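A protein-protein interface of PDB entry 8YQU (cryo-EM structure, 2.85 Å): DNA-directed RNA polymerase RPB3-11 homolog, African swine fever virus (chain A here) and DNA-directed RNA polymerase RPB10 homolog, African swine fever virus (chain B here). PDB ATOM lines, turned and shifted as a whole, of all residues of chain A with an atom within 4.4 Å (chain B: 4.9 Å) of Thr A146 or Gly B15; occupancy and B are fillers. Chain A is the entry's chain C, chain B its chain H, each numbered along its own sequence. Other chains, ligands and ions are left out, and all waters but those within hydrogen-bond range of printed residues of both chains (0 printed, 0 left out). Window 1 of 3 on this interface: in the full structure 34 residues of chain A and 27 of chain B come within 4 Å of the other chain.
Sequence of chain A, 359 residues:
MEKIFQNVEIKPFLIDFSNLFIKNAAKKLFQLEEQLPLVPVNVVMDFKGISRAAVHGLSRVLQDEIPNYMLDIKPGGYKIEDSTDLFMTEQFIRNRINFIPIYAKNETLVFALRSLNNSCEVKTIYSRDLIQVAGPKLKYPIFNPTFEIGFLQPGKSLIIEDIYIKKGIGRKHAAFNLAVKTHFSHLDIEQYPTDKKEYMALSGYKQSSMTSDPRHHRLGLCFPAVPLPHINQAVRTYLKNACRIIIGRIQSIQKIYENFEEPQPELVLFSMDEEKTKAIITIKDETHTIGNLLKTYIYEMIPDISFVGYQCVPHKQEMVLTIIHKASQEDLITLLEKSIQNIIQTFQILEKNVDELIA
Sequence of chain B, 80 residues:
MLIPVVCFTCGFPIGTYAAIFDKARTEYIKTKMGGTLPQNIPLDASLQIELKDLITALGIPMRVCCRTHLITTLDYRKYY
The side-chain amide nitrogen of Asn A144 lies close to the side-chain hydroxyl of Thr B16 (3.4 Å). OG1 of Thr A146 sits at hydrogen-bond distance from OG1 of Thr B16.
The side-chain hydroxyl (OG) of Ser A127 lies within hydrogen-bond range of the backbone carbonyl oxygen (O) of Asn A144 (2.5 Å). The side-chain hydroxyl of Ser A127 sits at hydrogen-bond distance from the backbone NH of Thr A146 (3.5 Å). The backbone NH (N) of Ser A127 sits at hydrogen-bond distance from the backbone carbonyl oxygen (O) of Phe A147 (3.0 Å). O of Pro B4 lies within hydrogen-bond range of N of Gly B15, at 3.4 Å. The backbone carbonyl oxygen of Val B5 sits at hydrogen-bond distance from the backbone NH of Ile B14 (3.1 Å). The backbone NH (N) of Gly B15 is in hydrogen-bond range of the backbone carbonyl oxygen (O) of Val B5 (2.5 Å).
Ala B19 touches Phe A30 (CB to CZ, 3.9 Å). Leu A36 touches Thr B16. Thr A146 touches Gly B15. Val B5 touches Phe A147 (CG1 to CE1, 3.5 Å). Phe A147 touches Gly B15. Phe A147 touches Thr B16. Glu A148 touches Ala B19.
Thr A146 touches just these residues of chain B: Gly B15 and Thr B16. Of chain A, only Thr A146 (3.8 Å) and Phe A147 (3.8 Å) come within 4 Å of Gly B15. Printed residues of chain B within 4 Å of Glu A148: Ala B19 (3.2 Å). Printed residues of chain B within 4 Å of Leu A36: Thr B16 (3.7 Å). Printed residues of chain A within 4 Å of Thr B16: Leu A36 (3.7 Å), Asn A144 (3.3 Å), Thr A146 (2.6 Å) and Phe A147 (3.4 Å). Printed residues of chain B within 4 Å of Phe A147: Val B5 (3.5 Å), Gly B15 (3.8 Å) and Thr B16 (3.4 Å). Tyr B17 touches none of the printed residues of chain A. The nearest printed residue of chain A that does not touch Gly B15 is Glu A148 (4.7 Å). The nearest printed residue of chain B that does not touch Leu A36 is Tyr B17 (4.3 Å).
Of the 8 printed residues of chain A, 6 touch a printed residue of chain B. Hydrophobic or aromatic side chains of chain A that line the printed part of chain B: Phe A30, Leu A36 and Phe A147. Of the 10 printed residues of chain B, 4 touch a printed residue of chain A. Among the printed residues, 9 pairs touch across the chains. Among the printed residues, no Asp or Glu carboxylate lies within 4 Å of a Lys or Arg side-chain nitrogen of the other chain.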
ATOM      1  N   PHE A  30      20.949  14.531 -27.002  1.00  0.00           N
ATOM      2  CA  PHE A  30      20.135  13.334 -26.830  1.00  0.00           C
ATOM      3  C   PHE A  30      18.651  13.597 -27.029  1.00  0.00           C
ATOM      4  O   PHE A  30      17.836  12.707 -26.766  1.00  0.00           O
ATOM      5  CB  PHE A  30      20.375  12.729 -25.445  1.00  0.00           C
ATOM      6  CG  PHE A  30      21.826  12.525 -25.117  1.00  0.00           C
ATOM      7  CD1 PHE A  30      22.546  11.502 -25.707  1.00  0.00           C
ATOM      8  CD2 PHE A  30      22.469  13.359 -24.219  1.00  0.00           C
ATOM      9  CE1 PHE A  30      23.881  11.314 -25.406  1.00  0.00           C
ATOM     10  CE2 PHE A  30      23.803  13.176 -23.914  1.00  0.00           C
ATOM     11  CZ  PHE A  30      24.509  12.152 -24.509  1.00  0.00           C
ATOM     12  N   LEU A  36      16.121  11.579 -16.755  1.00  0.00           N
ATOM     13  CA  LEU A  36      16.603  10.302 -17.248  1.00  0.00           C
ATOM     14  C   LEU A  36      15.860   9.154 -16.570  1.00  0.00           C
ATOM     15  O   LEU A  36      15.342   9.307 -15.461  1.00  0.00           O
ATOM     16  CB  LEU A  36      18.105  10.179 -17.006  1.00  0.00           C
ATOM     17  CG  LEU A  36      18.995  10.978 -17.960  1.00  0.00           C
ATOM     18  CD1 LEU A  36      20.447  10.927 -17.513  1.00  0.00           C
ATOM     19  CD2 LEU A  36      18.848  10.460 -19.379  1.00  0.00           C
ATOM     20  N   SER A 127      25.731   4.832 -25.009  1.00  0.00           N
ATOM     21  CA  SER A 127      25.123   3.644 -24.426  1.00  0.00           C
ATOM     22  C   SER A 127      23.723   3.370 -24.957  1.00  0.00           C
ATOM     23  O   SER A 127      23.189   2.284 -24.710  1.00  0.00           O
ATOM     24  CB  SER A 127      25.081   3.762 -22.903  1.00  0.00           C
ATOM     25  OG  SER A 127      24.179   4.771 -22.492  1.00  0.00           O
ATOM     26  N   ASN A 144      21.220   4.184 -18.243  1.00  0.00           N
ATOM     27  CA  ASN A 144      20.967   5.462 -18.888  1.00  0.00           C
ATOM     28  C   ASN A 144      21.528   5.458 -20.310  1.00  0.00           C
ATOM     29  O   ASN A 144      22.600   4.896 -20.554  1.00  0.00           O
ATOM     30  CB  ASN A 144      21.589   6.602 -18.084  1.00  0.00           C
ATOM     31  CG  ASN A 144      20.773   6.962 -16.861  1.00  0.00           C
ATOM     32  OD1 ASN A 144      19.548   7.047 -16.922  1.00  0.00           O
ATOM     33  ND2 ASN A 144      21.451   7.177 -15.741  1.00  0.00           N
ATOM     34  N   PRO A 145      20.832   6.072 -21.264  1.00  0.00           N
ATOM     35  CA  PRO A 145      21.319   6.124 -22.650  1.00  0.00           C
ATOM     36  C   PRO A 145      22.291   7.257 -22.952  1.00  0.00           C
ATOM     37  O   PRO A 145      22.553   7.511 -24.132  1.00  0.00           O
ATOM     38  CB  PRO A 145      20.020   6.318 -23.442  1.00  0.00           C
ATOM     39  CG  PRO A 145      19.152   7.092 -22.524  1.00  0.00           C
ATOM     40  CD  PRO A 145      19.461   6.598 -21.138  1.00  0.00           C
ATOM     41  N   THR A 146      22.830   7.937 -21.940  1.00  0.00           N
ATOM     42  CA  THR A 146      23.672   9.107 -22.148  1.00  0.00           C
ATOM     43  C   THR A 146      25.150   8.837 -21.893  1.00  0.00           C
ATOM     44  O   THR A 146      25.947   9.781 -21.879  1.00  0.00           O
ATOM     45  CB  THR A 146      23.198  10.260 -21.263  1.00  0.00           C
ATOM     46  OG1 THR A 146      23.240   9.857 -19.889  1.00  0.00           O
ATOM     47  CG2 THR A 146      21.778  10.657 -21.625  1.00  0.00           C
ATOM     48  N   PHE A 147      25.538   7.583 -21.688  1.00  0.00           N
ATOM     49  CA  PHE A 147      26.937   7.263 -21.451  1.00  0.00           C
ATOM     50  C   PHE A 147      27.728   7.343 -22.750  1.00  0.00           C
ATOM     51  O   PHE A 147      27.177   7.226 -23.845  1.00  0.00           O
ATOM     52  CB  PHE A 147      27.075   5.868 -20.844  1.00  0.00           C
ATOM     53  CG  PHE A 147      26.664   5.792 -19.405  1.00  0.00           C
ATOM     54  CD1 PHE A 147      27.535   6.177 -18.401  1.00  0.00           C
ATOM     55  CD2 PHE A 147      25.405   5.336 -19.057  1.00  0.00           C
ATOM     56  CE1 PHE A 147      27.156   6.108 -17.077  1.00  0.00           C
ATOM     57  CE2 PHE A 147      25.024   5.264 -17.734  1.00  0.00           C
ATOM     58  CZ  PHE A 147      25.900   5.650 -16.743  1.00  0.00           C
ATOM     59  N   GLU A 148      29.036   7.552 -22.617  1.00  0.00           N
ATOM     60  CA  GLU A 148      29.952   7.584 -23.757  1.00  0.00           C
ATOM     61  C   GLU A 148      30.775   6.302 -23.737  1.00  0.00           C
ATOM     62  O   GLU A 148      31.783   6.211 -23.032  1.00  0.00           O
ATOM     63  CB  GLU A 148      30.852   8.813 -23.710  1.00  0.00           C
ATOM     64  CG  GLU A 148      30.197  10.104 -24.163  1.00  0.00           C
ATOM     65  CD  GLU A 148      31.098  11.305 -23.961  1.00  0.00           C
ATOM     66  OE1 GLU A 148      31.981  11.245 -23.080  1.00  0.00           O
ATOM     67  OE2 GLU A 148      30.935  12.304 -24.691  1.00  0.00           O
ATOM     68  N   PRO B   4      35.649   9.556 -17.509  1.00  0.00           N
ATOM     69  CA  PRO B   4      35.334   8.202 -17.040  1.00  0.00           C
ATOM     70  C   PRO B   4      33.848   8.021 -16.775  1.00  0.00           C
ATOM     71  O   PRO B   4      33.131   8.969 -16.446  1.00  0.00           O
ATOM     72  CB  PRO B   4      36.151   8.075 -15.749  1.00  0.00           C
ATOM     73  CG  PRO B   4      36.383   9.480 -15.309  1.00  0.00           C
ATOM     74  CD  PRO B   4      36.521  10.277 -16.567  1.00  0.00           C
ATOM     75  N   VAL B   5      33.389   6.779 -16.940  1.00  0.00           N
ATOM     76  CA  VAL B   5      31.988   6.459 -16.685  1.00  0.00           C
ATOM     77  C   VAL B   5      31.635   6.741 -15.232  1.00  0.00           C
ATOM     78  O   VAL B   5      30.581   7.314 -14.931  1.00  0.00           O
ATOM     79  CB  VAL B   5      31.698   4.995 -17.064  1.00  0.00           C
ATOM     80  CG1 VAL B   5      30.307   4.596 -16.617  1.00  0.00           C
ATOM     81  CG2 VAL B   5      31.844   4.801 -18.557  1.00  0.00           C
ATOM     82  N   VAL B   6      32.512   6.351 -14.309  1.00  0.00           N
ATOM     83  CA  VAL B   6      32.322   6.606 -12.890  1.00  0.00           C
ATOM     84  C   VAL B   6      33.551   7.328 -12.357  1.00  0.00           C
ATOM     85  O   VAL B   6      34.646   7.239 -12.915  1.00  0.00           O
ATOM     86  CB  VAL B   6      32.067   5.312 -12.089  1.00  0.00           C
ATOM     87  CG1 VAL B   6      30.756   4.675 -12.514  1.00  0.00           C
ATOM     88  CG2 VAL B   6      33.220   4.343 -12.272  1.00  0.00           C
ATOM     89  N   PRO B  13      28.219   7.907 -10.766  1.00  0.00           N
ATOM     90  CA  PRO B  13      28.054   7.839 -12.226  1.00  0.00           C
ATOM     91  C   PRO B  13      28.266   9.181 -12.906  1.00  0.00           C
ATOM     92  O   PRO B  13      27.311   9.848 -13.313  1.00  0.00           O
ATOM     93  CB  PRO B  13      26.611   7.347 -12.395  1.00  0.00           C
ATOM     94  CG  PRO B  13      25.935   7.706 -11.119  1.00  0.00           C
ATOM     95  CD  PRO B  13      26.976   7.566 -10.055  1.00  0.00           C
ATOM     96  N   ILE B  14      29.532   9.582 -13.023  1.00  0.00           N
ATOM     97  CA  ILE B  14      29.873  10.837 -13.684  1.00  0.00           C
ATOM     98  C   ILE B  14      29.605  10.754 -15.181  1.00  0.00           C
ATOM     99  O   ILE B  14      29.192  11.739 -15.806  1.00  0.00           O
ATOM    100  CB  ILE B  14      31.338  11.201 -13.383  1.00  0.00           C
ATOM    101  CG1 ILE B  14      31.530  11.378 -11.880  1.00  0.00           C
ATOM    102  CG2 ILE B  14      31.746  12.455 -14.111  1.00  0.00           C
ATOM    103  CD1 ILE B  14      30.683  12.487 -11.311  1.00  0.00           C
ATOM    104  N   GLY B  15      29.827   9.581 -15.778  1.00  0.00           N
ATOM    105  CA  GLY B  15      29.767   9.465 -17.226  1.00  0.00           C
ATOM    106  C   GLY B  15      28.414   9.799 -17.822  1.00  0.00           C
ATOM    107  O   GLY B  15      28.338  10.331 -18.932  1.00  0.00           O
ATOM    108  N   THR B  16      27.330   9.496 -17.104  1.00  0.00           N
ATOM    109  CA  THR B  16      26.000   9.723 -17.657  1.00  0.00           C
ATOM    110  C   THR B  16      25.666  11.203 -17.804  1.00  0.00           C
ATOM    111  O   THR B  16      24.732  11.540 -18.538  1.00  0.00           O
ATOM    112  CB  THR B  16      24.942   9.022 -16.802  1.00  0.00           C
ATOM    113  OG1 THR B  16      23.661   9.134 -17.434  1.00  0.00           O
ATOM    114  CG2 THR B  16      24.882   9.621 -15.420  1.00  0.00           C
ATOM    115  N   TYR B  17      26.400  12.092 -17.134  1.00  0.00           N
ATOM    116  CA  TYR B  17      26.300  13.525 -17.387  1.00  0.00           C
ATOM    117  C   TYR B  17      27.578  14.078 -18.005  1.00  0.00           C
ATOM    118  O   TYR B  17      27.783  15.296 -18.012  1.00  0.00           O
ATOM    119  CB  TYR B  17      25.968  14.293 -16.106  1.00  0.00           C
ATOM    120  CG  TYR B  17      24.893  13.671 -15.248  1.00  0.00           C
ATOM    121  CD1 TYR B  17      23.553  13.963 -15.461  1.00  0.00           C
ATOM    122  CD2 TYR B  17      25.220  12.838 -14.189  1.00  0.00           C
ATOM    123  CE1 TYR B  17      22.568  13.405 -14.672  1.00  0.00           C
ATOM    124  CE2 TYR B  17      24.241  12.282 -13.389  1.00  0.00           C
ATOM    125  CZ  TYR B  17      22.918  12.568 -13.637  1.00  0.00           C
ATOM    126  OH  TYR B  17      21.937  12.017 -12.846  1.00  0.00           O
ATOM    127  N   ALA B  18      28.442  13.205 -18.521  1.00  0.00           N
ATOM    128  CA  ALA B  18      29.727  13.647 -19.051  1.00  0.00           C
ATOM    129  C   ALA B  18      29.553  14.404 -20.361  1.00  0.00           C
ATOM    130  O   ALA B  18      29.918  15.581 -20.465  1.00  0.00           O
ATOM    131  CB  ALA B  18      30.652  12.446 -19.242  1.00  0.00           C
ATOM    132  N   ALA B  19      28.979  13.739 -21.370  1.00  0.00           N
ATOM    133  CA  ALA B  19      28.882  14.322 -22.705  1.00  0.00           C
ATOM    134  C   ALA B  19      28.247  15.703 -22.661  1.00  0.00           C
ATOM    135  O   ALA B  19      28.811  16.677 -23.177  1.00  0.00           O
ATOM    136  CB  ALA B  19      28.085  13.394 -23.623  1.00  0.00           C
